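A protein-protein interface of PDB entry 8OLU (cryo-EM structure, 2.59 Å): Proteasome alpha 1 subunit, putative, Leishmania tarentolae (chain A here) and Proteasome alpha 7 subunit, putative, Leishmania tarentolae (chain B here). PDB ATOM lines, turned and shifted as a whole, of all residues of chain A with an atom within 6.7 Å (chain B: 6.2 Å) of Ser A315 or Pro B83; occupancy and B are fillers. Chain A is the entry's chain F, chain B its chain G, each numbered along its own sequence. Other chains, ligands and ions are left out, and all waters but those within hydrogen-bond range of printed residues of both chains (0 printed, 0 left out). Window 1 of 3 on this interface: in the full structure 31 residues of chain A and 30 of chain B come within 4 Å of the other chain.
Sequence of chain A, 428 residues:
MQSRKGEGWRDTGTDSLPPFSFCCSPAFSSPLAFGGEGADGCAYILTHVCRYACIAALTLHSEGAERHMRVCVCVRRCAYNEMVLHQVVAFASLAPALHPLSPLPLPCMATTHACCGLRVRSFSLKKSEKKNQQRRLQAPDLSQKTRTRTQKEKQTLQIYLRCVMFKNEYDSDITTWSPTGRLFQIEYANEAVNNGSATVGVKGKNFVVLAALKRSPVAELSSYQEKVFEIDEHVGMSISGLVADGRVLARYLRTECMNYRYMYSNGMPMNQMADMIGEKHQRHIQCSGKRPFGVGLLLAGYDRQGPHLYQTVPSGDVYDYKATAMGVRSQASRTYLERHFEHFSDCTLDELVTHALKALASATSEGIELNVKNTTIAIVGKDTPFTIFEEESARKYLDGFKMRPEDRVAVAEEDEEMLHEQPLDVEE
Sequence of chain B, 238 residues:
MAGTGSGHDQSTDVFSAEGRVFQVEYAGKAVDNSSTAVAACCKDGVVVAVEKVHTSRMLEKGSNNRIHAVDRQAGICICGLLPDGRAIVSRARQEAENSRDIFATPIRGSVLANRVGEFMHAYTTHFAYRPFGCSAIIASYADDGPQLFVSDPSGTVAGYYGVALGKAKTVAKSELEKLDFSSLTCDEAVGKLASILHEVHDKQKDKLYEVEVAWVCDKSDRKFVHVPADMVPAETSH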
ATOM      1  N   ILE A 186      -9.460 -18.906   5.435  1.00  0.00           N
ATOM      2  CA  ILE A 186     -10.868 -18.612   5.527  1.00  0.00           C
ATOM      3  C   ILE A 186     -11.078 -17.205   5.999  1.00  0.00           C
ATOM      4  O   ILE A 186     -12.060 -16.653   5.582  1.00  0.00           O
ATOM      5  CB  ILE A 186     -11.609 -19.577   6.454  1.00  0.00           C
ATOM      6  CG1 ILE A 186     -11.658 -20.948   5.818  1.00  0.00           C
ATOM      7  CG2 ILE A 186     -13.014 -19.095   6.802  1.00  0.00           C
ATOM      8  CD1 ILE A 186     -12.332 -21.924   6.693  1.00  0.00           C
ATOM      9  N   ALA A 189     -10.617 -15.198   2.606  1.00  0.00           N
ATOM     10  CA  ALA A 189     -11.833 -15.280   1.851  1.00  0.00           C
ATOM     11  C   ALA A 189     -12.899 -14.378   2.430  1.00  0.00           C
ATOM     12  O   ALA A 189     -13.731 -13.898   1.692  1.00  0.00           O
ATOM     13  CB  ALA A 189     -12.317 -16.666   1.886  1.00  0.00           C
ATOM     14  N   ASN A 190     -12.942 -14.178   3.733  1.00  0.00           N
ATOM     15  CA  ASN A 190     -13.951 -13.290   4.268  1.00  0.00           C
ATOM     16  C   ASN A 190     -13.678 -11.889   3.791  1.00  0.00           C
ATOM     17  O   ASN A 190     -14.599 -11.125   3.628  1.00  0.00           O
ATOM     18  CB  ASN A 190     -13.985 -13.247   5.794  1.00  0.00           C
ATOM     19  CG  ASN A 190     -15.092 -14.122   6.315  1.00  0.00           C
ATOM     20  OD1 ASN A 190     -15.103 -15.345   6.120  1.00  0.00           O
ATOM     21  ND2 ASN A 190     -16.087 -13.450   6.874  1.00  0.00           N
ATOM     22  N   GLY A 278     -24.431 -24.433   2.660  1.00  0.00           N
ATOM     23  CA  GLY A 278     -23.415 -24.412   3.689  1.00  0.00           C
ATOM     24  C   GLY A 278     -22.520 -25.631   3.649  1.00  0.00           C
ATOM     25  O   GLY A 278     -21.402 -25.565   4.080  1.00  0.00           O
ATOM     26  N   GLU A 279     -23.048 -26.755   3.223  1.00  0.00           N
ATOM     27  CA  GLU A 279     -22.301 -27.985   3.063  1.00  0.00           C
ATOM     28  C   GLU A 279     -21.394 -27.837   1.847  1.00  0.00           C
ATOM     29  O   GLU A 279     -20.300 -28.371   1.842  1.00  0.00           O
ATOM     30  CB  GLU A 279     -23.273 -29.155   2.967  1.00  0.00           C
ATOM     31  CG  GLU A 279     -22.590 -30.531   2.945  1.00  0.00           C
ATOM     32  CD  GLU A 279     -21.942 -31.124   4.219  1.00  0.00           C
ATOM     33  OE1 GLU A 279     -20.642 -31.184   4.293  1.00  0.00           O
ATOM     34  OE2 GLU A 279     -22.717 -31.602   5.125  1.00  0.00           O
ATOM     35  N   HIS A 281     -19.971 -25.118   0.822  1.00  0.00           N
ATOM     36  CA  HIS A 281     -18.860 -24.335   1.287  1.00  0.00           C
ATOM     37  C   HIS A 281     -17.913 -25.173   2.116  1.00  0.00           C
ATOM     38  O   HIS A 281     -16.726 -24.915   2.114  1.00  0.00           O
ATOM     39  CB  HIS A 281     -19.375 -23.186   2.123  1.00  0.00           C
ATOM     40  CG  HIS A 281     -19.906 -22.025   1.358  1.00  0.00           C
ATOM     41  ND1 HIS A 281     -21.130 -21.972   0.805  1.00  0.00           N
ATOM     42  CD2 HIS A 281     -19.392 -20.781   1.230  1.00  0.00           C
ATOM     43  CE1 HIS A 281     -21.371 -20.736   0.367  1.00  0.00           C
ATOM     44  NE2 HIS A 281     -20.291 -19.979   0.582  1.00  0.00           N
ATOM     45  N   GLN A 282     -18.418 -26.099   2.908  1.00  0.00           N
ATOM     46  CA  GLN A 282     -17.513 -26.770   3.799  1.00  0.00           C
ATOM     47  C   GLN A 282     -16.610 -27.696   3.035  1.00  0.00           C
ATOM     48  O   GLN A 282     -15.540 -28.028   3.477  1.00  0.00           O
ATOM     49  CB  GLN A 282     -18.221 -27.640   4.822  1.00  0.00           C
ATOM     50  CG  GLN A 282     -17.323 -27.924   6.046  1.00  0.00           C
ATOM     51  CD  GLN A 282     -16.631 -29.269   5.990  1.00  0.00           C
ATOM     52  OE1 GLN A 282     -16.961 -30.155   5.203  1.00  0.00           O
ATOM     53  NE2 GLN A 282     -15.616 -29.398   6.837  1.00  0.00           N
ATOM     54  N   ILE A 285     -13.343 -26.035   2.323  1.00  0.00           N
ATOM     55  CA  ILE A 285     -12.424 -25.499   3.298  1.00  0.00           C
ATOM     56  C   ILE A 285     -11.691 -26.564   4.084  1.00  0.00           C
ATOM     57  O   ILE A 285     -11.150 -26.271   5.131  1.00  0.00           O
ATOM     58  CB  ILE A 285     -13.142 -24.553   4.242  1.00  0.00           C
ATOM     59  CG1 ILE A 285     -14.230 -25.271   5.035  1.00  0.00           C
ATOM     60  CG2 ILE A 285     -13.689 -23.410   3.457  1.00  0.00           C
ATOM     61  CD1 ILE A 285     -14.581 -24.598   6.359  1.00  0.00           C
ATOM     62  N   PRO A 292     -11.799 -21.810  -0.349  1.00  0.00           N
ATOM     63  CA  PRO A 292     -13.059 -21.217   0.051  1.00  0.00           C
ATOM     64  C   PRO A 292     -13.606 -20.404  -1.108  1.00  0.00           C
ATOM     65  O   PRO A 292     -12.865 -19.904  -1.948  1.00  0.00           O
ATOM     66  CB  PRO A 292     -12.703 -20.345   1.246  1.00  0.00           C
ATOM     67  CG  PRO A 292     -11.335 -20.842   1.672  1.00  0.00           C
ATOM     68  CD  PRO A 292     -10.660 -21.377   0.435  1.00  0.00           C
ATOM     69  N   PHE A 293     -14.925 -20.371  -1.189  1.00  0.00           N
ATOM     70  CA  PHE A 293     -15.631 -19.391  -1.980  1.00  0.00           C
ATOM     71  C   PHE A 293     -15.377 -18.023  -1.385  1.00  0.00           C
ATOM     72  O   PHE A 293     -15.385 -17.845  -0.179  1.00  0.00           O
ATOM     73  CB  PHE A 293     -17.109 -19.719  -1.945  1.00  0.00           C
ATOM     74  CG  PHE A 293     -17.384 -20.973  -2.711  1.00  0.00           C
ATOM     75  CD1 PHE A 293     -17.269 -20.984  -4.084  1.00  0.00           C
ATOM     76  CD2 PHE A 293     -17.676 -22.153  -2.062  1.00  0.00           C
ATOM     77  CE1 PHE A 293     -17.517 -22.135  -4.799  1.00  0.00           C
ATOM     78  CE2 PHE A 293     -17.909 -23.313  -2.785  1.00  0.00           C
ATOM     79  CZ  PHE A 293     -17.827 -23.296  -4.151  1.00  0.00           C
ATOM     80  N   THR A 312     -24.769 -16.133   3.974  1.00  0.00           N
ATOM     81  CA  THR A 312     -23.760 -17.163   4.013  1.00  0.00           C
ATOM     82  C   THR A 312     -22.405 -16.525   3.821  1.00  0.00           C
ATOM     83  O   THR A 312     -22.283 -15.436   3.271  1.00  0.00           O
ATOM     84  CB  THR A 312     -23.813 -18.144   2.839  1.00  0.00           C
ATOM     85  OG1 THR A 312     -23.044 -17.587   1.756  1.00  0.00           O
ATOM     86  CG2 THR A 312     -25.232 -18.474   2.417  1.00  0.00           C
ATOM     87  N   VAL A 313     -21.395 -17.265   4.229  1.00  0.00           N
ATOM     88  CA  VAL A 313     -20.050 -16.747   4.228  1.00  0.00           C
ATOM     89  C   VAL A 313     -19.081 -17.841   3.816  1.00  0.00           C
ATOM     90  O   VAL A 313     -19.383 -19.034   3.762  1.00  0.00           O
ATOM     91  CB  VAL A 313     -19.721 -16.175   5.608  1.00  0.00           C
ATOM     92  CG1 VAL A 313     -20.459 -14.862   5.834  1.00  0.00           C
ATOM     93  CG2 VAL A 313     -20.089 -17.206   6.665  1.00  0.00           C
ATOM     94  N   PRO A 314     -17.884 -17.434   3.408  1.00  0.00           N
ATOM     95  CA  PRO A 314     -16.898 -18.410   2.952  1.00  0.00           C
ATOM     96  C   PRO A 314     -16.666 -19.567   3.917  1.00  0.00           C
ATOM     97  O   PRO A 314     -16.452 -20.683   3.462  1.00  0.00           O
ATOM     98  CB  PRO A 314     -15.686 -17.500   2.857  1.00  0.00           C
ATOM     99  CG  PRO A 314     -16.316 -16.213   2.375  1.00  0.00           C
ATOM    100  CD  PRO A 314     -17.465 -16.031   3.318  1.00  0.00           C
ATOM    101  N   SER A 315     -16.757 -19.291   5.219  1.00  0.00           N
ATOM    102  CA  SER A 315     -16.453 -20.257   6.254  1.00  0.00           C
ATOM    103  C   SER A 315     -17.403 -21.426   6.223  1.00  0.00           C
ATOM    104  O   SER A 315     -17.141 -22.406   6.880  1.00  0.00           O
ATOM    105  CB  SER A 315     -16.541 -19.652   7.631  1.00  0.00           C
ATOM    106  OG  SER A 315     -17.902 -19.483   8.039  1.00  0.00           O
ATOM    107  N   GLY A 316     -18.542 -21.252   5.564  1.00  0.00           N
ATOM    108  CA  GLY A 316     -19.576 -22.261   5.446  1.00  0.00           C
ATOM    109  C   GLY A 316     -20.738 -22.011   6.406  1.00  0.00           C
ATOM    110  O   GLY A 316     -21.689 -22.784   6.459  1.00  0.00           O
ATOM    111  N   ASP A 317     -20.614 -20.988   7.223  1.00  0.00           N
ATOM    112  CA  ASP A 317     -21.674 -20.672   8.139  1.00  0.00           C
ATOM    113  C   ASP A 317     -22.844 -20.096   7.382  1.00  0.00           C
ATOM    114  O   ASP A 317     -22.685 -19.490   6.336  1.00  0.00           O
ATOM    115  CB  ASP A 317     -21.234 -19.642   9.140  1.00  0.00           C
ATOM    116  CG  ASP A 317     -20.513 -20.303  10.283  1.00  0.00           C
ATOM    117  OD1 ASP A 317     -19.244 -20.123  10.372  1.00  0.00           O
ATOM    118  OD2 ASP A 317     -21.231 -21.010  11.077  1.00  0.00           O
ATOM    119  N   VAL A 318     -24.024 -20.312   7.926  1.00  0.00           N
ATOM    120  CA  VAL A 318     -25.228 -19.796   7.352  1.00  0.00           C
ATOM    121  C   VAL A 318     -26.048 -19.234   8.479  1.00  0.00           C
ATOM    122  O   VAL A 318     -26.405 -19.941   9.401  1.00  0.00           O
ATOM    123  CB  VAL A 318     -25.975 -20.932   6.679  1.00  0.00           C
ATOM    124  CG1 VAL A 318     -27.266 -20.419   6.097  1.00  0.00           C
ATOM    125  CG2 VAL A 318     -25.139 -21.580   5.592  1.00  0.00           C
ATOM    126  N   TYR A 319     -26.368 -17.977   8.378  1.00  0.00           N
ATOM    127  CA  TYR A 319     -27.092 -17.293   9.420  1.00  0.00           C
ATOM    128  C   TYR A 319     -28.508 -17.110   8.926  1.00  0.00           C
ATOM    129  O   TYR A 319     -28.689 -16.933   7.741  1.00  0.00           O
ATOM    130  CB  TYR A 319     -26.371 -15.989   9.698  1.00  0.00           C
ATOM    131  CG  TYR A 319     -24.942 -16.176  10.125  1.00  0.00           C
ATOM    132  CD1 TYR A 319     -24.627 -16.475  11.439  1.00  0.00           C
ATOM    133  CD2 TYR A 319     -23.894 -16.085   9.213  1.00  0.00           C
ATOM    134  CE1 TYR A 319     -23.310 -16.657  11.849  1.00  0.00           C
ATOM    135  CE2 TYR A 319     -22.564 -16.240   9.616  1.00  0.00           C
ATOM    136  CZ  TYR A 319     -22.271 -16.523  10.943  1.00  0.00           C
ATOM    137  OH  TYR A 319     -20.990 -16.734  11.355  1.00  0.00           O
ATOM    138  N   GLY B  80     -17.295 -25.898  18.514  1.00  0.00           N
ATOM    139  CA  GLY B  80     -16.210 -25.482  17.638  1.00  0.00           C
ATOM    140  C   GLY B  80     -16.762 -24.960  16.328  1.00  0.00           C
ATOM    141  O   GLY B  80     -17.874 -24.464  16.297  1.00  0.00           O
ATOM    142  N   LEU B  81     -16.035 -25.121  15.244  1.00  0.00           N
ATOM    143  CA  LEU B  81     -16.499 -24.588  13.981  1.00  0.00           C
ATOM    144  C   LEU B  81     -17.758 -25.269  13.488  1.00  0.00           C
ATOM    145  O   LEU B  81     -17.748 -26.365  12.959  1.00  0.00           O
ATOM    146  CB  LEU B  81     -15.455 -24.772  12.890  1.00  0.00           C
ATOM    147  CG  LEU B  81     -14.160 -24.007  13.085  1.00  0.00           C
ATOM    148  CD1 LEU B  81     -13.482 -23.972  11.726  1.00  0.00           C
ATOM    149  CD2 LEU B  81     -14.363 -22.602  13.702  1.00  0.00           C
ATOM    150  N   LEU B  82     -18.810 -24.492  13.471  1.00  0.00           N
ATOM    151  CA  LEU B  82     -20.064 -25.082  13.151  1.00  0.00           C
ATOM    152  C   LEU B  82     -20.066 -25.731  11.780  1.00  0.00           C
ATOM    153  O   LEU B  82     -20.617 -26.818  11.599  1.00  0.00           O
ATOM    154  CB  LEU B  82     -21.134 -24.023  13.289  1.00  0.00           C
ATOM    155  CG  LEU B  82     -22.538 -24.581  13.179  1.00  0.00           C
ATOM    156  CD1 LEU B  82     -22.697 -25.772  14.119  1.00  0.00           C
ATOM    157  CD2 LEU B  82     -23.543 -23.489  13.498  1.00  0.00           C
ATOM    158  N   PRO B  83     -19.526 -25.127  10.735  1.00  0.00           N
ATOM    159  CA  PRO B  83     -19.530 -25.789   9.428  1.00  0.00           C
ATOM    160  C   PRO B  83     -18.858 -27.161   9.370  1.00  0.00           C
ATOM    161  O   PRO B  83     -19.373 -28.072   8.730  1.00  0.00           O
ATOM    162  CB  PRO B  83     -18.685 -24.818   8.615  1.00  0.00           C
ATOM    163  CG  PRO B  83     -19.000 -23.510   9.233  1.00  0.00           C
ATOM    164  CD  PRO B  83     -18.954 -23.787  10.719  1.00  0.00           C
ATOM    165  N   ASP B  84     -17.691 -27.271  10.023  1.00  0.00           N
ATOM    166  CA  ASP B  84     -17.006 -28.536  10.172  1.00  0.00           C
ATOM    167  C   ASP B  84     -17.904 -29.531  10.883  1.00  0.00           C
ATOM    168  O   ASP B  84     -17.947 -30.706  10.548  1.00  0.00           O
ATOM    169  CB  ASP B  84     -15.700 -28.387  10.937  1.00  0.00           C
ATOM    170  CG  ASP B  84     -14.478 -28.228  10.042  1.00  0.00           C
ATOM    171  OD1 ASP B  84     -14.648 -28.243   8.792  1.00  0.00           O
ATOM    172  OD2 ASP B  84     -13.349 -28.132  10.581  1.00  0.00           O
ATOM    173  N   GLY B  85     -18.626 -29.074  11.870  1.00  0.00           N
ATOM    174  CA  GLY B  85     -19.529 -29.972  12.541  1.00  0.00           C
ATOM    175  C   GLY B  85     -20.665 -30.418  11.638  1.00  0.00           C
ATOM    176  O   GLY B  85     -21.168 -31.527  11.753  1.00  0.00           O
ATOM    177  N   ARG B  86     -21.167 -29.540  10.807  1.00  0.00           N
ATOM    178  CA  ARG B  86     -22.249 -30.000   9.988  1.00  0.00           C
ATOM    179  C   ARG B  86     -21.687 -31.056   9.048  1.00  0.00           C
ATOM    180  O   ARG B  86     -22.403 -31.915   8.540  1.00  0.00           O
ATOM    181  CB  ARG B  86     -22.984 -28.801   9.384  1.00  0.00           C
ATOM    182  CG  ARG B  86     -23.649 -27.954  10.473  1.00  0.00           C
ATOM    183  CD  ARG B  86     -24.677 -26.927  10.024  1.00  0.00           C
ATOM    184  NE  ARG B  86     -25.602 -27.590   9.092  1.00  0.00           N
ATOM    185  CZ  ARG B  86     -26.909 -27.765   9.274  1.00  0.00           C
ATOM    186  NH1 ARG B  86     -27.471 -28.924   8.981  1.00  0.00           N
ATOM    187  NH2 ARG B  86     -27.638 -26.795   9.781  1.00  0.00           N
ATOM    188  N   ALA B  87     -20.387 -31.090   8.858  1.00  0.00           N
ATOM    189  CA  ALA B  87     -19.874 -32.145   8.026  1.00  0.00           C
ATOM    190  C   ALA B  87     -19.894 -33.483   8.744  1.00  0.00           C
ATOM    191  O   ALA B  87     -19.990 -34.535   8.106  1.00  0.00           O
ATOM    192  CB  ALA B  87     -18.490 -31.830   7.625  1.00  0.00           C
ATOM    193  N   ILE B  88     -19.634 -33.430  10.028  1.00  0.00           N
ATOM    194  CA  ILE B  88     -19.671 -34.600  10.856  1.00  0.00           C
ATOM    195  C   ILE B  88     -21.075 -35.101  11.037  1.00  0.00           C
ATOM    196  O   ILE B  88     -21.326 -36.281  10.918  1.00  0.00           O
ATOM    197  CB  ILE B  88     -19.064 -34.227  12.192  1.00  0.00           C
ATOM    198  CG1 ILE B  88     -17.572 -34.080  11.955  1.00  0.00           C
ATOM    199  CG2 ILE B  88     -19.345 -35.274  13.253  1.00  0.00           C
ATOM    200  CD1 ILE B  88     -16.930 -33.420  13.124  1.00  0.00           C
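The backbone carbonyl oxygen (O) of Arg B86 lies close to the side-chain carboxylate (OE2) of Glu A279 (3.4 Å). OD1 of Asp B84 lies within hydrogen-bond range of NE2 of Gln A282, 2.5 Å away.
Printed residues of chain A that touch a printed residue of chain B: Glu A279, Gln A282, Ser A315, Gly A316 and Asp A317. Among the printed residues, 9 pairs touch across the chains. Among the printed residues, no Asp or Glu carboxylate lies within 4 Å of a Lys or Arg side-chain nitrogen of the other chain.
Ser A315 touches just one residue of chain B: Pro B83. Pro B83 touches just these residues of chain A: Gln A282, Ser A315, Gly A316 and Asp A317. Printed residues of chain B within 4 Å of Asp A317: Leu B82 and Pro B83. Of the printed residues of chain A, Asp B84 touches Gln A282 (2.5 Å). Pro A292 touches none of the printed residues of chain B. Phe A293 touches none of the printed residues of chain B. The nearest residue of chain A that does not touch Pro B83 is Ile A285 (4.7 Å).
OG of Ser A315 lies within hydrogen-bond range of OD1 of Asp A317 (2.8 Å).
Among the printed residues, pairs that only touch across the chains: Glu A279 with Ala B87, Gln A282 with Pro B83, Gln A282 with Ala B87, Ser A315 with Pro B83, Gly A316 with Pro B83, Asp A317 with Leu B82 and Asp A317 with Pro B83.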
